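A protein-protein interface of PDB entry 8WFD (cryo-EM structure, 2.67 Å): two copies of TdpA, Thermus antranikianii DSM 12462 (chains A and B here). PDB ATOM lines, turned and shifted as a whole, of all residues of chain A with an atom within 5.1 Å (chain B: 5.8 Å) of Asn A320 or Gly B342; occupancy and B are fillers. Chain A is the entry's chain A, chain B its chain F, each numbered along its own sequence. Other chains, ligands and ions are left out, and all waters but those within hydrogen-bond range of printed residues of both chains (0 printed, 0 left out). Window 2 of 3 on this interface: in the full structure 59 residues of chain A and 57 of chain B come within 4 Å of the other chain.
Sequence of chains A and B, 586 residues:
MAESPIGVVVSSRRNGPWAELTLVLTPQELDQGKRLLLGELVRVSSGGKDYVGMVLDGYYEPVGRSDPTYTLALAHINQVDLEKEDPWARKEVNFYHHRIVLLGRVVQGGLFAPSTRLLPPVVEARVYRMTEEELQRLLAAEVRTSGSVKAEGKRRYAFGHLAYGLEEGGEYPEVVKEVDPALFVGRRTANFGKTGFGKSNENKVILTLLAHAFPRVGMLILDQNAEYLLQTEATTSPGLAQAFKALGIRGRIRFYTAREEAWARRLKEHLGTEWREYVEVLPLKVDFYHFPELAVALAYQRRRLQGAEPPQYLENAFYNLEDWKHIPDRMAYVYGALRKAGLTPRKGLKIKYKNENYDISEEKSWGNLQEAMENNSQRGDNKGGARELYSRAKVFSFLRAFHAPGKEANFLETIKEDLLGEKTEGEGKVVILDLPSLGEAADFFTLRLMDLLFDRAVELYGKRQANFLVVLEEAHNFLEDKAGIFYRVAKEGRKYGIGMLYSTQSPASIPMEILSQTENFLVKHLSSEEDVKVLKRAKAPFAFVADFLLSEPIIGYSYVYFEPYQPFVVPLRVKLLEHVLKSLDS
Tyr A319 touches Ser B397.
Asn A320 touches Gly B342.
NH1 of Arg B400 lies within hydrogen-bond range of O of Gly B342, at 3.2 Å.
OD1 of Asn A316 lies within hydrogen-bond range of ND2 of Asn A320.
Gly B342 touches just one residue of chain A: Asn A320 (3.4 Å).
Of the printed residues of chain A, Arg B400 touches Tyr A319 (3.0 Å), Asn A320 (3.3 Å), Glu A322 (3.3 Å) and Asp A323 (2.9 Å).
Printed residues of chain B within 4 Å of Glu A322: Arg B400 (3.3 Å).
Printed residues of chain B within 4 Å of Asn A316: Ala B341 and Ser B397.
Of the printed residues of chain A, Ser B397 touches Asn A316 (2.6 Å) and Tyr A319 (3.9 Å).
Of the printed residues of chain A, Ala B341 touches Asn A316 and Asn A320.
Lys B340 touches none of the printed residues of chain A.
Trp A324 touches none of the printed residues of chain B.
The nearest residue of chain A that does not touch Gly B342 is Asp A323 (4.4 Å).
The side-chain carboxylate of Asp A323 lies within salt-bridge range of the guanidinium group of Arg B400.
NE of Arg B400 sits at hydrogen-bond distance from OD1 of Asn A320.
The guanidinium group (NE) of Arg B400 sits at hydrogen-bond distance from the backbone carbonyl oxygen (O) of Tyr A319 (3.0 Å).
The side-chain amide oxygen (OD1) of Asn A316 is in hydrogen-bond range of the side-chain hydroxyl (OG) of Ser B397, 2.6 Å away.
NH2 of Arg B400 is in salt-bridge range of OE2 of Glu A322 (3.3 Å).
The backbone carbonyl oxygen of Ala B341 lies close to the side-chain amide oxygen of Asn A316 (3.5 Å).
ND2 of Asn A320 is in hydrogen-bond range of O of Ala B341, at 3.1 Å.
Of the 10 printed residues of chain B, 4 touch a printed residue of chain A.
Printed residues of chain B that touch a printed residue of chain A: Ala B341, Gly B342, Ser B397 and Arg B400.
Among the printed residues, 9 pairs touch across the chains.
No position is printed for both chains.
Of the 9 pairs that touch across the chains among the printed residues, none has its exchanged pair printed and touching as well.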
ATOM      1  N   GLU A 315      10.685   9.428  -7.311  1.00  0.00           N
ATOM      2  CA  GLU A 315      11.793   9.490  -8.259  1.00  0.00           C
ATOM      3  C   GLU A 315      11.304   9.801  -9.667  1.00  0.00           C
ATOM      4  O   GLU A 315      11.954  10.561 -10.396  1.00  0.00           O
ATOM      5  CB  GLU A 315      12.575   8.180  -8.245  1.00  0.00           C
ATOM      6  CG  GLU A 315      13.039   7.759  -6.867  1.00  0.00           C
ATOM      7  CD  GLU A 315      13.942   6.547  -6.898  1.00  0.00           C
ATOM      8  OE1 GLU A 315      13.438   5.434  -7.154  1.00  0.00           O
ATOM      9  OE2 GLU A 315      15.158   6.705  -6.665  1.00  0.00           O
ATOM     10  N   ASN A 316      10.170   9.224 -10.065  1.00  0.00           N
ATOM     11  CA  ASN A 316       9.613   9.508 -11.382  1.00  0.00           C
ATOM     12  C   ASN A 316       9.369  11.000 -11.561  1.00  0.00           C
ATOM     13  O   ASN A 316       9.823  11.604 -12.540  1.00  0.00           O
ATOM     14  CB  ASN A 316       8.317   8.720 -11.572  1.00  0.00           C
ATOM     15  CG  ASN A 316       7.984   8.485 -13.026  1.00  0.00           C
ATOM     16  OD1 ASN A 316       8.870   8.291 -13.855  1.00  0.00           O
ATOM     17  ND2 ASN A 316       6.699   8.494 -13.344  1.00  0.00           N
ATOM     18  N   ALA A 317       8.655  11.616 -10.616  1.00  0.00           N
ATOM     19  CA  ALA A 317       8.391  13.046 -10.711  1.00  0.00           C
ATOM     20  C   ALA A 317       9.681  13.849 -10.662  1.00  0.00           C
ATOM     21  O   ALA A 317       9.874  14.767 -11.467  1.00  0.00           O
ATOM     22  CB  ALA A 317       7.443  13.479  -9.596  1.00  0.00           C
ATOM     23  N   PHE A 318      10.588  13.496  -9.748  1.00  0.00           N
ATOM     24  CA  PHE A 318      11.847  14.221  -9.617  1.00  0.00           C
ATOM     25  C   PHE A 318      12.594  14.266 -10.940  1.00  0.00           C
ATOM     26  O   PHE A 318      13.117  15.314 -11.335  1.00  0.00           O
ATOM     27  CB  PHE A 318      12.703  13.566  -8.531  1.00  0.00           C
ATOM     28  CG  PHE A 318      14.019  14.248  -8.294  1.00  0.00           C
ATOM     29  CD1 PHE A 318      14.072  15.497  -7.700  1.00  0.00           C
ATOM     30  CD2 PHE A 318      15.205  13.634  -8.654  1.00  0.00           C
ATOM     31  CE1 PHE A 318      15.282  16.120  -7.479  1.00  0.00           C
ATOM     32  CE2 PHE A 318      16.415  14.255  -8.435  1.00  0.00           C
ATOM     33  CZ  PHE A 318      16.455  15.497  -7.848  1.00  0.00           C
ATOM     34  N   TYR A 319      12.658  13.139 -11.643  1.00  0.00           N
ATOM     35  CA  TYR A 319      13.427  13.073 -12.876  1.00  0.00           C
ATOM     36  C   TYR A 319      12.649  13.505 -14.113  1.00  0.00           C
ATOM     37  O   TYR A 319      13.270  13.751 -15.152  1.00  0.00           O
ATOM     38  CB  TYR A 319      13.963  11.655 -13.088  1.00  0.00           C
ATOM     39  CG  TYR A 319      15.161  11.320 -12.231  1.00  0.00           C
ATOM     40  CD1 TYR A 319      16.387  11.928 -12.451  1.00  0.00           C
ATOM     41  CD2 TYR A 319      15.064  10.399 -11.201  1.00  0.00           C
ATOM     42  CE1 TYR A 319      17.480  11.626 -11.671  1.00  0.00           C
ATOM     43  CE2 TYR A 319      16.152  10.092 -10.415  1.00  0.00           C
ATOM     44  CZ  TYR A 319      17.357  10.708 -10.653  1.00  0.00           C
ATOM     45  OH  TYR A 319      18.444  10.400  -9.870  1.00  0.00           O
ATOM     46  N   ASN A 320      11.319  13.611 -14.047  1.00  0.00           N
ATOM     47  CA  ASN A 320      10.536  13.837 -15.252  1.00  0.00           C
ATOM     48  C   ASN A 320       9.667  15.089 -15.247  1.00  0.00           C
ATOM     49  O   ASN A 320       9.010  15.356 -16.260  1.00  0.00           O
ATOM     50  CB  ASN A 320       9.639  12.621 -15.528  1.00  0.00           C
ATOM     51  CG  ASN A 320      10.401  11.465 -16.136  1.00  0.00           C
ATOM     52  OD1 ASN A 320      10.926  11.568 -17.243  1.00  0.00           O
ATOM     53  ND2 ASN A 320      10.474  10.358 -15.411  1.00  0.00           N
ATOM     54  N   LEU A 321       9.628  15.861 -14.159  1.00  0.00           N
ATOM     55  CA  LEU A 321       8.759  17.031 -14.150  1.00  0.00           C
ATOM     56  C   LEU A 321       9.183  18.082 -15.169  1.00  0.00           C
ATOM     57  O   LEU A 321       8.326  18.803 -15.694  1.00  0.00           O
ATOM     58  CB  LEU A 321       8.710  17.641 -12.750  1.00  0.00           C
ATOM     59  CG  LEU A 321       7.642  18.719 -12.563  1.00  0.00           C
ATOM     60  CD1 LEU A 321       7.012  18.620 -11.188  1.00  0.00           C
ATOM     61  CD2 LEU A 321       8.244  20.093 -12.772  1.00  0.00           C
ATOM     62  N   GLU A 322      10.480  18.183 -15.468  1.00  0.00           N
ATOM     63  CA  GLU A 322      10.926  19.123 -16.490  1.00  0.00           C
ATOM     64  C   GLU A 322      10.293  18.804 -17.840  1.00  0.00           C
ATOM     65  O   GLU A 322       9.857  19.709 -18.559  1.00  0.00           O
ATOM     66  CB  GLU A 322      12.451  19.101 -16.593  1.00  0.00           C
ATOM     67  CG  GLU A 322      13.017  17.778 -17.092  1.00  0.00           C
ATOM     68  CD  GLU A 322      14.531  17.774 -17.174  1.00  0.00           C
ATOM     69  OE1 GLU A 322      15.158  18.761 -16.736  1.00  0.00           O
ATOM     70  OE2 GLU A 322      15.095  16.782 -17.684  1.00  0.00           O
ATOM     71  N   ASP A 323      10.245  17.520 -18.204  1.00  0.00           N
ATOM     72  CA  ASP A 323       9.532  17.122 -19.413  1.00  0.00           C
ATOM     73  C   ASP A 323       8.036  17.365 -19.274  1.00  0.00           C
ATOM     74  O   ASP A 323       7.388  17.837 -20.214  1.00  0.00           O
ATOM     75  CB  ASP A 323       9.805  15.653 -19.729  1.00  0.00           C
ATOM     76  CG  ASP A 323      11.239  15.400 -20.145  1.00  0.00           C
ATOM     77  OD1 ASP A 323      11.950  16.374 -20.469  1.00  0.00           O
ATOM     78  OD2 ASP A 323      11.654  14.223 -20.153  1.00  0.00           O
ATOM     79  N   TRP A 324       7.470  17.044 -18.108  1.00  0.00           N
ATOM     80  CA  TRP A 324       6.032  17.211 -17.914  1.00  0.00           C
ATOM     81  C   TRP A 324       5.585  18.654 -18.090  1.00  0.00           C
ATOM     82  O   TRP A 324       4.441  18.889 -18.489  1.00  0.00           O
ATOM     83  CB  TRP A 324       5.612  16.722 -16.527  1.00  0.00           C
ATOM     84  CG  TRP A 324       5.814  15.263 -16.305  1.00  0.00           C
ATOM     85  CD1 TRP A 324       6.143  14.330 -17.239  1.00  0.00           C
ATOM     86  CD2 TRP A 324       5.689  14.563 -15.064  1.00  0.00           C
ATOM     87  NE1 TRP A 324       6.240  13.092 -16.655  1.00  0.00           N
ATOM     88  CE2 TRP A 324       5.964  13.209 -15.319  1.00  0.00           C
ATOM     89  CE3 TRP A 324       5.376  14.954 -13.760  1.00  0.00           C
ATOM     90  CZ2 TRP A 324       5.934  12.243 -14.320  1.00  0.00           C
ATOM     91  CZ3 TRP A 324       5.348  13.997 -12.774  1.00  0.00           C
ATOM     92  CH2 TRP A 324       5.625  12.657 -13.055  1.00  0.00           C
ATOM     93  N   ALA B 337       8.445  -0.062 -21.619  1.00  0.00           N
ATOM     94  CA  ALA B 337       8.729   0.253 -20.224  1.00  0.00           C
ATOM     95  C   ALA B 337       9.805   1.322 -20.116  1.00  0.00           C
ATOM     96  O   ALA B 337       9.686   2.258 -19.315  1.00  0.00           O
ATOM     97  CB  ALA B 337       9.147  -1.009 -19.473  1.00  0.00           C
ATOM     98  N   LEU B 338      10.864   1.209 -20.921  1.00  0.00           N
ATOM     99  CA  LEU B 338      11.893   2.245 -20.907  1.00  0.00           C
ATOM    100  C   LEU B 338      11.324   3.597 -21.317  1.00  0.00           C
ATOM    101  O   LEU B 338      11.640   4.620 -20.701  1.00  0.00           O
ATOM    102  CB  LEU B 338      13.058   1.860 -21.816  1.00  0.00           C
ATOM    103  CG  LEU B 338      13.929   0.686 -21.373  1.00  0.00           C
ATOM    104  CD1 LEU B 338      15.056   0.462 -22.363  1.00  0.00           C
ATOM    105  CD2 LEU B 338      14.476   0.931 -19.982  1.00  0.00           C
ATOM    106  N   ARG B 339      10.484   3.624 -22.354  1.00  0.00           N
ATOM    107  CA  ARG B 339       9.926   4.889 -22.824  1.00  0.00           C
ATOM    108  C   ARG B 339       8.936   5.472 -21.821  1.00  0.00           C
ATOM    109  O   ARG B 339       8.828   6.695 -21.685  1.00  0.00           O
ATOM    110  CB  ARG B 339       9.256   4.693 -24.183  1.00  0.00           C
ATOM    111  CG  ARG B 339       8.556   5.929 -24.715  1.00  0.00           C
ATOM    112  CD  ARG B 339       9.547   6.897 -25.322  1.00  0.00           C
ATOM    113  NE  ARG B 339       8.903   7.859 -26.206  1.00  0.00           N
ATOM    114  CZ  ARG B 339       8.441   9.039 -25.820  1.00  0.00           C
ATOM    115  NH1 ARG B 339       8.526   9.437 -24.561  1.00  0.00           N
ATOM    116  NH2 ARG B 339       7.882   9.843 -26.719  1.00  0.00           N
ATOM    117  N   LYS B 340       8.196   4.613 -21.120  1.00  0.00           N
ATOM    118  CA  LYS B 340       7.220   5.081 -20.148  1.00  0.00           C
ATOM    119  C   LYS B 340       7.892   5.580 -18.877  1.00  0.00           C
ATOM    120  O   LYS B 340       7.366   6.477 -18.212  1.00  0.00           O
ATOM    121  CB  LYS B 340       6.233   3.960 -19.828  1.00  0.00           C
ATOM    122  CG  LYS B 340       4.974   4.413 -19.120  1.00  0.00           C
ATOM    123  CD  LYS B 340       4.419   3.312 -18.238  1.00  0.00           C
ATOM    124  CE  LYS B 340       3.323   2.535 -18.941  1.00  0.00           C
ATOM    125  NZ  LYS B 340       2.527   1.719 -17.983  1.00  0.00           N
ATOM    126  N   ALA B 341       9.044   5.011 -18.522  1.00  0.00           N
ATOM    127  CA  ALA B 341       9.788   5.483 -17.363  1.00  0.00           C
ATOM    128  C   ALA B 341      10.391   6.865 -17.568  1.00  0.00           C
ATOM    129  O   ALA B 341      10.850   7.472 -16.595  1.00  0.00           O
ATOM    130  CB  ALA B 341      10.892   4.488 -17.006  1.00  0.00           C
ATOM    131  N   GLY B 342      10.404   7.376 -18.798  1.00  0.00           N
ATOM    132  CA  GLY B 342      10.875   8.714 -19.087  1.00  0.00           C
ATOM    133  C   GLY B 342      12.129   8.784 -19.929  1.00  0.00           C
ATOM    134  O   GLY B 342      12.535   9.890 -20.303  1.00  0.00           O
ATOM    135  N   LEU B 343      12.749   7.652 -20.247  1.00  0.00           N
ATOM    136  CA  LEU B 343      13.994   7.664 -21.003  1.00  0.00           C
ATOM    137  C   LEU B 343      13.752   8.145 -22.427  1.00  0.00           C
ATOM    138  O   LEU B 343      12.858   7.650 -23.120  1.00  0.00           O
ATOM    139  CB  LEU B 343      14.618   6.271 -21.011  1.00  0.00           C
ATOM    140  CG  LEU B 343      15.496   5.901 -19.815  1.00  0.00           C
ATOM    141  CD1 LEU B 343      14.734   6.030 -18.513  1.00  0.00           C
ATOM    142  CD2 LEU B 343      16.034   4.495 -19.977  1.00  0.00           C
ATOM    143  N   THR B 344      14.555   9.107 -22.863  1.00  0.00           N
ATOM    144  CA  THR B 344      14.399   9.695 -24.190  1.00  0.00           C
ATOM    145  C   THR B 344      15.103   8.834 -25.235  1.00  0.00           C
ATOM    146  O   THR B 344      16.285   8.520 -25.074  1.00  0.00           O
ATOM    147  CB  THR B 344      14.969  11.110 -24.218  1.00  0.00           C
ATOM    148  OG1 THR B 344      14.312  11.912 -23.229  1.00  0.00           O
ATOM    149  CG2 THR B 344      14.764  11.739 -25.584  1.00  0.00           C
ATOM    150  N   SER B 397      12.815   4.592 -13.408  1.00  0.00           N
ATOM    151  CA  SER B 397      12.985   6.039 -13.452  1.00  0.00           C
ATOM    152  C   SER B 397      14.385   6.454 -13.015  1.00  0.00           C
ATOM    153  O   SER B 397      14.973   7.374 -13.594  1.00  0.00           O
ATOM    154  CB  SER B 397      11.928   6.715 -12.581  1.00  0.00           C
ATOM    155  OG  SER B 397      10.641   6.572 -13.150  1.00  0.00           O
ATOM    156  N   ARG B 400      17.333   7.189 -15.287  1.00  0.00           N
ATOM    157  CA  ARG B 400      17.420   8.453 -16.000  1.00  0.00           C
ATOM    158  C   ARG B 400      18.589   9.301 -15.528  1.00  0.00           C
ATOM    159  O   ARG B 400      18.900  10.310 -16.169  1.00  0.00           O
ATOM    160  CB  ARG B 400      16.100   9.209 -15.846  1.00  0.00           C
ATOM    161  CG  ARG B 400      15.949  10.413 -16.747  1.00  0.00           C
ATOM    162  CD  ARG B 400      14.484  10.669 -17.037  1.00  0.00           C
ATOM    163  NE  ARG B 400      14.232  12.045 -17.442  1.00  0.00           N
ATOM    164  CZ  ARG B 400      14.499  12.535 -18.644  1.00  0.00           C
ATOM    165  NH1 ARG B 400      15.043  11.787 -19.590  1.00  0.00           N
ATOM    166  NH2 ARG B 400      14.214  13.806 -18.904  1.00  0.00           N
